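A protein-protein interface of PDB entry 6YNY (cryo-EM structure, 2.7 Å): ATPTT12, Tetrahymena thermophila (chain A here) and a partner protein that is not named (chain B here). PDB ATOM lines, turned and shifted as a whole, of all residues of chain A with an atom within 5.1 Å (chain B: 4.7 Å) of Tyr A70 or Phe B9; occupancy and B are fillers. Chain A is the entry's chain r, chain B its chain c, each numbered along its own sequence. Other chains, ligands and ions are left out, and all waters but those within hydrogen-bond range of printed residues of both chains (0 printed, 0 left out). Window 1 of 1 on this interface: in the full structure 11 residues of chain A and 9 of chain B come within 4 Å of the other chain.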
ATOM      1  N   ALA A  66      14.222  20.772   3.021  1.00  0.00           N
ATOM      2  CA  ALA A  66      14.513  22.169   3.305  1.00  0.00           C
ATOM      3  C   ALA A  66      15.789  22.317   4.119  1.00  0.00           C
ATOM      4  O   ALA A  66      16.482  23.334   4.006  1.00  0.00           O
ATOM      5  CB  ALA A  66      13.336  22.806   4.035  1.00  0.00           C
ATOM      6  N   VAL A  67      16.115  21.320   4.941  1.00  0.00           N
ATOM      7  CA  VAL A  67      17.353  21.364   5.709  1.00  0.00           C
ATOM      8  C   VAL A  67      18.555  21.262   4.781  1.00  0.00           C
ATOM      9  O   VAL A  67      19.537  21.998   4.931  1.00  0.00           O
ATOM     10  CB  VAL A  67      17.355  20.250   6.769  1.00  0.00           C
ATOM     11  CG1 VAL A  67      18.733  20.061   7.340  1.00  0.00           C
ATOM     12  CG2 VAL A  67      16.393  20.578   7.873  1.00  0.00           C
ATOM     13  N   ASP A  68      18.501  20.349   3.813  1.00  0.00           N
ATOM     14  CA  ASP A  68      19.590  20.223   2.854  1.00  0.00           C
ATOM     15  C   ASP A  68      19.705  21.467   1.984  1.00  0.00           C
ATOM     16  O   ASP A  68      20.812  21.881   1.624  1.00  0.00           O
ATOM     17  CB  ASP A  68      19.376  18.980   1.997  1.00  0.00           C
ATOM     18  CG  ASP A  68      19.496  17.697   2.794  1.00  0.00           C
ATOM     19  OD1 ASP A  68      18.648  17.464   3.681  1.00  0.00           O
ATOM     20  OD2 ASP A  68      20.438  16.921   2.537  1.00  0.00           O
ATOM     21  N   LYS A  69      18.572  22.074   1.638  1.00  0.00           N
ATOM     22  CA  LYS A  69      18.590  23.330   0.900  1.00  0.00           C
ATOM     23  C   LYS A  69      19.165  24.459   1.744  1.00  0.00           C
ATOM     24  O   LYS A  69      19.806  25.371   1.211  1.00  0.00           O
ATOM     25  CB  LYS A  69      17.173  23.662   0.443  1.00  0.00           C
ATOM     26  CG  LYS A  69      17.006  24.981  -0.272  1.00  0.00           C
ATOM     27  CD  LYS A  69      17.731  24.997  -1.591  1.00  0.00           C
ATOM     28  CE  LYS A  69      17.468  26.289  -2.339  1.00  0.00           C
ATOM     29  NZ  LYS A  69      16.023  26.478  -2.641  1.00  0.00           N
ATOM     30  N   TYR A  70      18.946  24.411   3.056  1.00  0.00           N
ATOM     31  CA  TYR A  70      19.417  25.454   3.955  1.00  0.00           C
ATOM     32  C   TYR A  70      20.905  25.331   4.234  1.00  0.00           C
ATOM     33  O   TYR A  70      21.587  26.345   4.407  1.00  0.00           O
ATOM     34  CB  TYR A  70      18.620  25.383   5.256  1.00  0.00           C
ATOM     35  CG  TYR A  70      19.050  26.337   6.341  1.00  0.00           C
ATOM     36  CD1 TYR A  70      18.726  27.680   6.278  1.00  0.00           C
ATOM     37  CD2 TYR A  70      19.751  25.885   7.445  1.00  0.00           C
ATOM     38  CE1 TYR A  70      19.106  28.547   7.272  1.00  0.00           C
ATOM     39  CE2 TYR A  70      20.132  26.745   8.441  1.00  0.00           C
ATOM     40  CZ  TYR A  70      19.807  28.074   8.353  1.00  0.00           C
ATOM     41  OH  TYR A  70      20.190  28.934   9.351  1.00  0.00           O
ATOM     42  N   ILE A  71      21.419  24.108   4.281  1.00  0.00           N
ATOM     43  CA  ILE A  71      22.811  23.867   4.633  1.00  0.00           C
ATOM     44  C   ILE A  71      23.695  23.803   3.397  1.00  0.00           C
ATOM     45  O   ILE A  71      24.702  24.507   3.303  1.00  0.00           O
ATOM     46  CB  ILE A  71      22.915  22.574   5.466  1.00  0.00           C
ATOM     47  CG1 ILE A  71      22.138  22.729   6.771  1.00  0.00           C
ATOM     48  CG2 ILE A  71      24.357  22.237   5.738  1.00  0.00           C
ATOM     49  CD1 ILE A  71      22.010  21.472   7.559  1.00  0.00           C
ATOM     50  N   PHE A  72      23.334  22.964   2.430  1.00  0.00           N
ATOM     51  CA  PHE A  72      24.162  22.757   1.252  1.00  0.00           C
ATOM     52  C   PHE A  72      23.905  23.793   0.167  1.00  0.00           C
ATOM     53  O   PHE A  72      24.848  24.258  -0.479  1.00  0.00           O
ATOM     54  CB  PHE A  72      23.922  21.359   0.688  1.00  0.00           C
ATOM     55  CG  PHE A  72      24.236  20.260   1.647  1.00  0.00           C
ATOM     56  CD1 PHE A  72      25.529  19.814   1.808  1.00  0.00           C
ATOM     57  CD2 PHE A  72      23.234  19.664   2.383  1.00  0.00           C
ATOM     58  CE1 PHE A  72      25.817  18.802   2.689  1.00  0.00           C
ATOM     59  CE2 PHE A  72      23.518  18.652   3.262  1.00  0.00           C
ATOM     60  CZ  PHE A  72      24.811  18.220   3.415  1.00  0.00           C
ATOM     61  N   GLY A  73      22.652  24.158  -0.048  1.00  0.00           N
ATOM     62  CA  GLY A  73      22.317  25.153  -1.039  1.00  0.00           C
ATOM     63  C   GLY A  73      21.954  24.540  -2.376  1.00  0.00           C
ATOM     64  O   GLY A  73      21.552  23.379  -2.490  1.00  0.00           O
ATOM     65  N   GLY A  79      24.362  27.012   1.791  1.00  0.00           N
ATOM     66  CA  GLY A  79      23.152  27.797   1.686  1.00  0.00           C
ATOM     67  C   GLY A  79      23.099  28.952   2.659  1.00  0.00           C
ATOM     68  O   GLY A  79      24.135  29.450   3.107  1.00  0.00           O
ATOM     69  N   LYS A  80      21.884  29.383   2.998  1.00  0.00           N
ATOM     70  CA  LYS A  80      21.703  30.488   3.926  1.00  0.00           C
ATOM     71  C   LYS A  80      22.256  30.186   5.309  1.00  0.00           C
ATOM     72  O   LYS A  80      22.401  31.110   6.116  1.00  0.00           O
ATOM     73  CB  LYS A  80      20.222  30.838   4.024  1.00  0.00           C
ATOM     74  CG  LYS A  80      19.640  31.381   2.739  1.00  0.00           C
ATOM     75  CD  LYS A  80      18.175  31.736   2.896  1.00  0.00           C
ATOM     76  CE  LYS A  80      17.588  32.229   1.586  1.00  0.00           C
ATOM     77  NZ  LYS A  80      16.135  32.515   1.681  1.00  0.00           N
ATOM     78  N   PHE A  81      22.571  28.924   5.599  1.00  0.00           N
ATOM     79  CA  PHE A  81      23.187  28.585   6.875  1.00  0.00           C
ATOM     80  C   PHE A  81      24.494  29.336   7.081  1.00  0.00           C
ATOM     81  O   PHE A  81      24.882  29.604   8.223  1.00  0.00           O
ATOM     82  CB  PHE A  81      23.416  27.077   6.945  1.00  0.00           C
ATOM     83  CG  PHE A  81      24.319  26.650   8.056  1.00  0.00           C
ATOM     84  CD1 PHE A  81      25.565  26.131   7.780  1.00  0.00           C
ATOM     85  CD2 PHE A  81      23.925  26.764   9.373  1.00  0.00           C
ATOM     86  CE1 PHE A  81      26.398  25.735   8.791  1.00  0.00           C
ATOM     87  CE2 PHE A  81      24.756  26.368  10.390  1.00  0.00           C
ATOM     88  CZ  PHE A  81      25.995  25.853  10.099  1.00  0.00           C
ATOM     89  N   LEU B   5      10.393  24.681   0.039  1.00  0.00           N
ATOM     90  CA  LEU B   5      10.667  26.092  -0.163  1.00  0.00           C
ATOM     91  C   LEU B   5      11.421  26.684   1.023  1.00  0.00           C
ATOM     92  O   LEU B   5      11.487  26.110   2.112  1.00  0.00           O
ATOM     93  CB  LEU B   5       9.368  26.862  -0.392  1.00  0.00           C
ATOM     94  CG  LEU B   5       8.836  26.825  -1.824  1.00  0.00           C
ATOM     95  CD1 LEU B   5       7.473  27.480  -1.903  1.00  0.00           C
ATOM     96  CD2 LEU B   5       9.814  27.505  -2.770  1.00  0.00           C
ATOM     97  N   ASP B   6      12.001  27.859   0.783  1.00  0.00           N
ATOM     98  CA  ASP B   6      12.777  28.562   1.792  1.00  0.00           C
ATOM     99  C   ASP B   6      11.912  29.184   2.876  1.00  0.00           C
ATOM    100  O   ASP B   6      12.456  29.657   3.878  1.00  0.00           O
ATOM    101  CB  ASP B   6      13.617  29.639   1.115  1.00  0.00           C
ATOM    102  CG  ASP B   6      14.540  29.073   0.059  1.00  0.00           C
ATOM    103  OD1 ASP B   6      14.030  28.506  -0.930  1.00  0.00           O
ATOM    104  OD2 ASP B   6      15.773  29.196   0.213  1.00  0.00           O
ATOM    105  N   TYR B   7      10.590  29.203   2.703  1.00  0.00           N
ATOM    106  CA  TYR B   7       9.727  29.747   3.742  1.00  0.00           C
ATOM    107  C   TYR B   7       9.785  28.907   5.008  1.00  0.00           C
ATOM    108  O   TYR B   7       9.539  29.421   6.104  1.00  0.00           O
ATOM    109  CB  TYR B   7       8.289  29.841   3.237  1.00  0.00           C
ATOM    110  CG  TYR B   7       8.113  30.742   2.038  1.00  0.00           C
ATOM    111  CD1 TYR B   7       8.170  32.122   2.169  1.00  0.00           C
ATOM    112  CD2 TYR B   7       7.878  30.213   0.778  1.00  0.00           C
ATOM    113  CE1 TYR B   7       8.008  32.948   1.079  1.00  0.00           C
ATOM    114  CE2 TYR B   7       7.713  31.033  -0.318  1.00  0.00           C
ATOM    115  CZ  TYR B   7       7.778  32.399  -0.163  1.00  0.00           C
ATOM    116  OH  TYR B   7       7.613  33.217  -1.255  1.00  0.00           O
ATOM    117  N   LEU B   8      10.106  27.620   4.881  1.00  0.00           N
ATOM    118  CA  LEU B   8      10.196  26.748   6.042  1.00  0.00           C
ATOM    119  C   LEU B   8      11.428  27.021   6.888  1.00  0.00           C
ATOM    120  O   LEU B   8      11.540  26.461   7.983  1.00  0.00           O
ATOM    121  CB  LEU B   8      10.195  25.289   5.599  1.00  0.00           C
ATOM    122  CG  LEU B   8       8.911  24.793   4.944  1.00  0.00           C
ATOM    123  CD1 LEU B   8       9.092  23.373   4.483  1.00  0.00           C
ATOM    124  CD2 LEU B   8       7.742  24.897   5.908  1.00  0.00           C
ATOM    125  N   PHE B   9      12.351  27.857   6.414  1.00  0.00           N
ATOM    126  CA  PHE B   9      13.521  28.191   7.214  1.00  0.00           C
ATOM    127  C   PHE B   9      13.137  28.922   8.489  1.00  0.00           C
ATOM    128  O   PHE B   9      13.944  28.993   9.421  1.00  0.00           O
ATOM    129  CB  PHE B   9      14.497  29.045   6.403  1.00  0.00           C
ATOM    130  CG  PHE B   9      15.022  28.372   5.163  1.00  0.00           C
ATOM    131  CD1 PHE B   9      14.699  27.061   4.867  1.00  0.00           C
ATOM    132  CD2 PHE B   9      15.853  29.054   4.296  1.00  0.00           C
ATOM    133  CE1 PHE B   9      15.184  26.454   3.733  1.00  0.00           C
ATOM    134  CE2 PHE B   9      16.340  28.446   3.163  1.00  0.00           C
ATOM    135  CZ  PHE B   9      16.006  27.146   2.884  1.00  0.00           C
ATOM    136  N   LEU B  10      11.922  29.465   8.550  1.00  0.00           N
ATOM    137  CA  LEU B  10      11.439  30.134   9.748  1.00  0.00           C
ATOM    138  C   LEU B  10      11.310  29.191  10.932  1.00  0.00           C
ATOM    139  O   LEU B  10      11.174  29.662  12.065  1.00  0.00           O
ATOM    140  CB  LEU B  10      10.088  30.781   9.460  1.00  0.00           C
ATOM    141  CG  LEU B  10      10.060  31.731   8.265  1.00  0.00           C
ATOM    142  CD1 LEU B  10       8.663  32.277   8.064  1.00  0.00           C
ATOM    143  CD2 LEU B  10      11.054  32.859   8.445  1.00  0.00           C
ATOM    144  N   LEU B  11      11.345  27.882  10.699  1.00  0.00           N
ATOM    145  CA  LEU B  11      11.269  26.908  11.774  1.00  0.00           C
ATOM    146  C   LEU B  11      12.581  26.753  12.529  1.00  0.00           C
ATOM    147  O   LEU B  11      12.607  26.076  13.560  1.00  0.00           O
ATOM    148  CB  LEU B  11      10.846  25.554  11.211  1.00  0.00           C
ATOM    149  CG  LEU B  11       9.529  25.537  10.436  1.00  0.00           C
ATOM    150  CD1 LEU B  11       9.282  24.179   9.827  1.00  0.00           C
ATOM    151  CD2 LEU B  11       8.374  25.925  11.326  1.00  0.00           C
ATOM    152  N   ASP B  12      13.659  27.363  12.051  1.00  0.00           N
ATOM    153  CA  ASP B  12      14.964  27.194  12.668  1.00  0.00           C
ATOM    154  C   ASP B  12      15.085  28.021  13.939  1.00  0.00           C
ATOM    155  O   ASP B  12      14.692  29.189  13.983  1.00  0.00           O
ATOM    156  CB  ASP B  12      16.070  27.591  11.694  1.00  0.00           C
ATOM    157  CG  ASP B  12      17.452  27.275  12.222  1.00  0.00           C
ATOM    158  OD1 ASP B  12      17.840  26.090  12.210  1.00  0.00           O
ATOM    159  OD2 ASP B  12      18.150  28.214  12.655  1.00  0.00           O
ATOM    160  N   ASP B  15      20.095  28.404  14.736  1.00  0.00           N
ATOM    161  CA  ASP B  15      20.907  29.463  14.154  1.00  0.00           C
ATOM    162  C   ASP B  15      20.155  30.786  14.105  1.00  0.00           C
ATOM    163  O   ASP B  15      20.432  31.635  13.258  1.00  0.00           O
ATOM    164  CB  ASP B  15      21.369  29.062  12.757  1.00  0.00           C
ATOM    165  CG  ASP B  15      22.138  27.758  12.752  1.00  0.00           C
ATOM    166  OD1 ASP B  15      23.002  27.571  13.633  1.00  0.00           O
ATOM    167  OD2 ASP B  15      21.870  26.913  11.872  1.00  0.00           O
ATOM    168  N   ARG B  19      20.406  35.795  12.480  1.00  0.00           N
ATOM    169  CA  ARG B  19      19.535  36.752  11.813  1.00  0.00           C
ATOM    170  C   ARG B  19      19.019  37.844  12.742  1.00  0.00           C
ATOM    171  O   ARG B  19      19.289  39.023  12.505  1.00  0.00           O
ATOM    172  CB  ARG B  19      18.347  36.015  11.179  1.00  0.00           C
ATOM    173  CG  ARG B  19      18.660  35.249   9.902  1.00  0.00           C
ATOM    174  CD  ARG B  19      18.832  33.770  10.133  1.00  0.00           C
ATOM    175  NE  ARG B  19      17.688  33.172  10.806  1.00  0.00           N
ATOM    176  CZ  ARG B  19      17.582  31.879  11.088  1.00  0.00           C
ATOM    177  NH1 ARG B  19      18.543  31.035  10.747  1.00  0.00           N
ATOM    178  NH2 ARG B  19      16.507  31.429  11.710  1.00  0.00           N
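The backbone carbonyl oxygen (O) of Tyr A70 sits at hydrogen-bond distance from the backbone NH (N) of Lys A80 (3.4 Å).
The backbone NH (N) of Phe A81 is in hydrogen-bond range of the backbone carbonyl oxygen (O) of Tyr A70 (3.0 Å).
OD2 of Asp B12 is in hydrogen-bond range of N of Asp B15, at 2.9 Å.
The guanidinium group (NH1) of Arg B19 lies within salt-bridge range of the side-chain carboxylate (OD2) of Asp B12, 3.4 Å away.
O of Asp B15 sits at hydrogen-bond distance from NH1 of Arg B19 (3.2 Å).
Printed residues of chain B within 4 Å of Ala A66: Phe B9.
Asp A68 touches none of the printed residues of chain B.
Of the printed residues of chain B, Lys A69 touches Asp B6 and Phe B9.
Of the printed residues of chain B, Lys A80 touches Asp B6 (3.6 Å) and Phe B9 (3.8 Å).
Printed residues of chain A within 4 Å of Asp B6: Lys A69 (3.3 Å) and Lys A80 (3.6 Å).
Leu B8 touches none of the printed residues of chain A.
Printed residues of chain A within 4 Å of Arg B19: Tyr A70 (3.0 Å).
The nearest printed residue of chain A that does not touch Phe B9 is Val A67 (5.4 Å).
The nearest printed residue of chain B that does not touch Phe A81 is Arg B19 (6.5 Å).
OD1 of Asp B6 lies within salt-bridge range of NZ of Lys A69, at 3.3 Å.
OH of Tyr A70 sits at hydrogen-bond distance from NH1 of Arg B19.
NZ of Lys A80 lies within salt-bridge range of OD2 of Asp B6, 3.6 Å away.
Among the printed residues, merely in contact across the chains: Ala A66 with Phe B9 (3.4 Å), Lys A69 with Phe B9 (3.96 Å), Tyr A70 with Phe B9 (3.8 Å), Tyr A70 with Asp B12 (3.9 Å), Tyr A70 with Asp B15 (3.6 Å), Lys A80 with Phe B9 (3.8 Å) and Phe A81 with Asp B15 (3.2 Å).
Hydrophobic or aromatic side chains of chain A within 4 Å of the printed part of chain B: Tyr A70 and Phe A81.
Of the 10 printed residues of chain B, 5 touch a printed residue of chain A.
Among the printed residues, 10 pairs touch across the chains.
Among the printed residues, Asp or Glu carboxylates within 4 Å of a Lys or Arg side-chain nitrogen of the other chain: Lys A69 with Asp B6 and Lys A80 with Asp B6.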
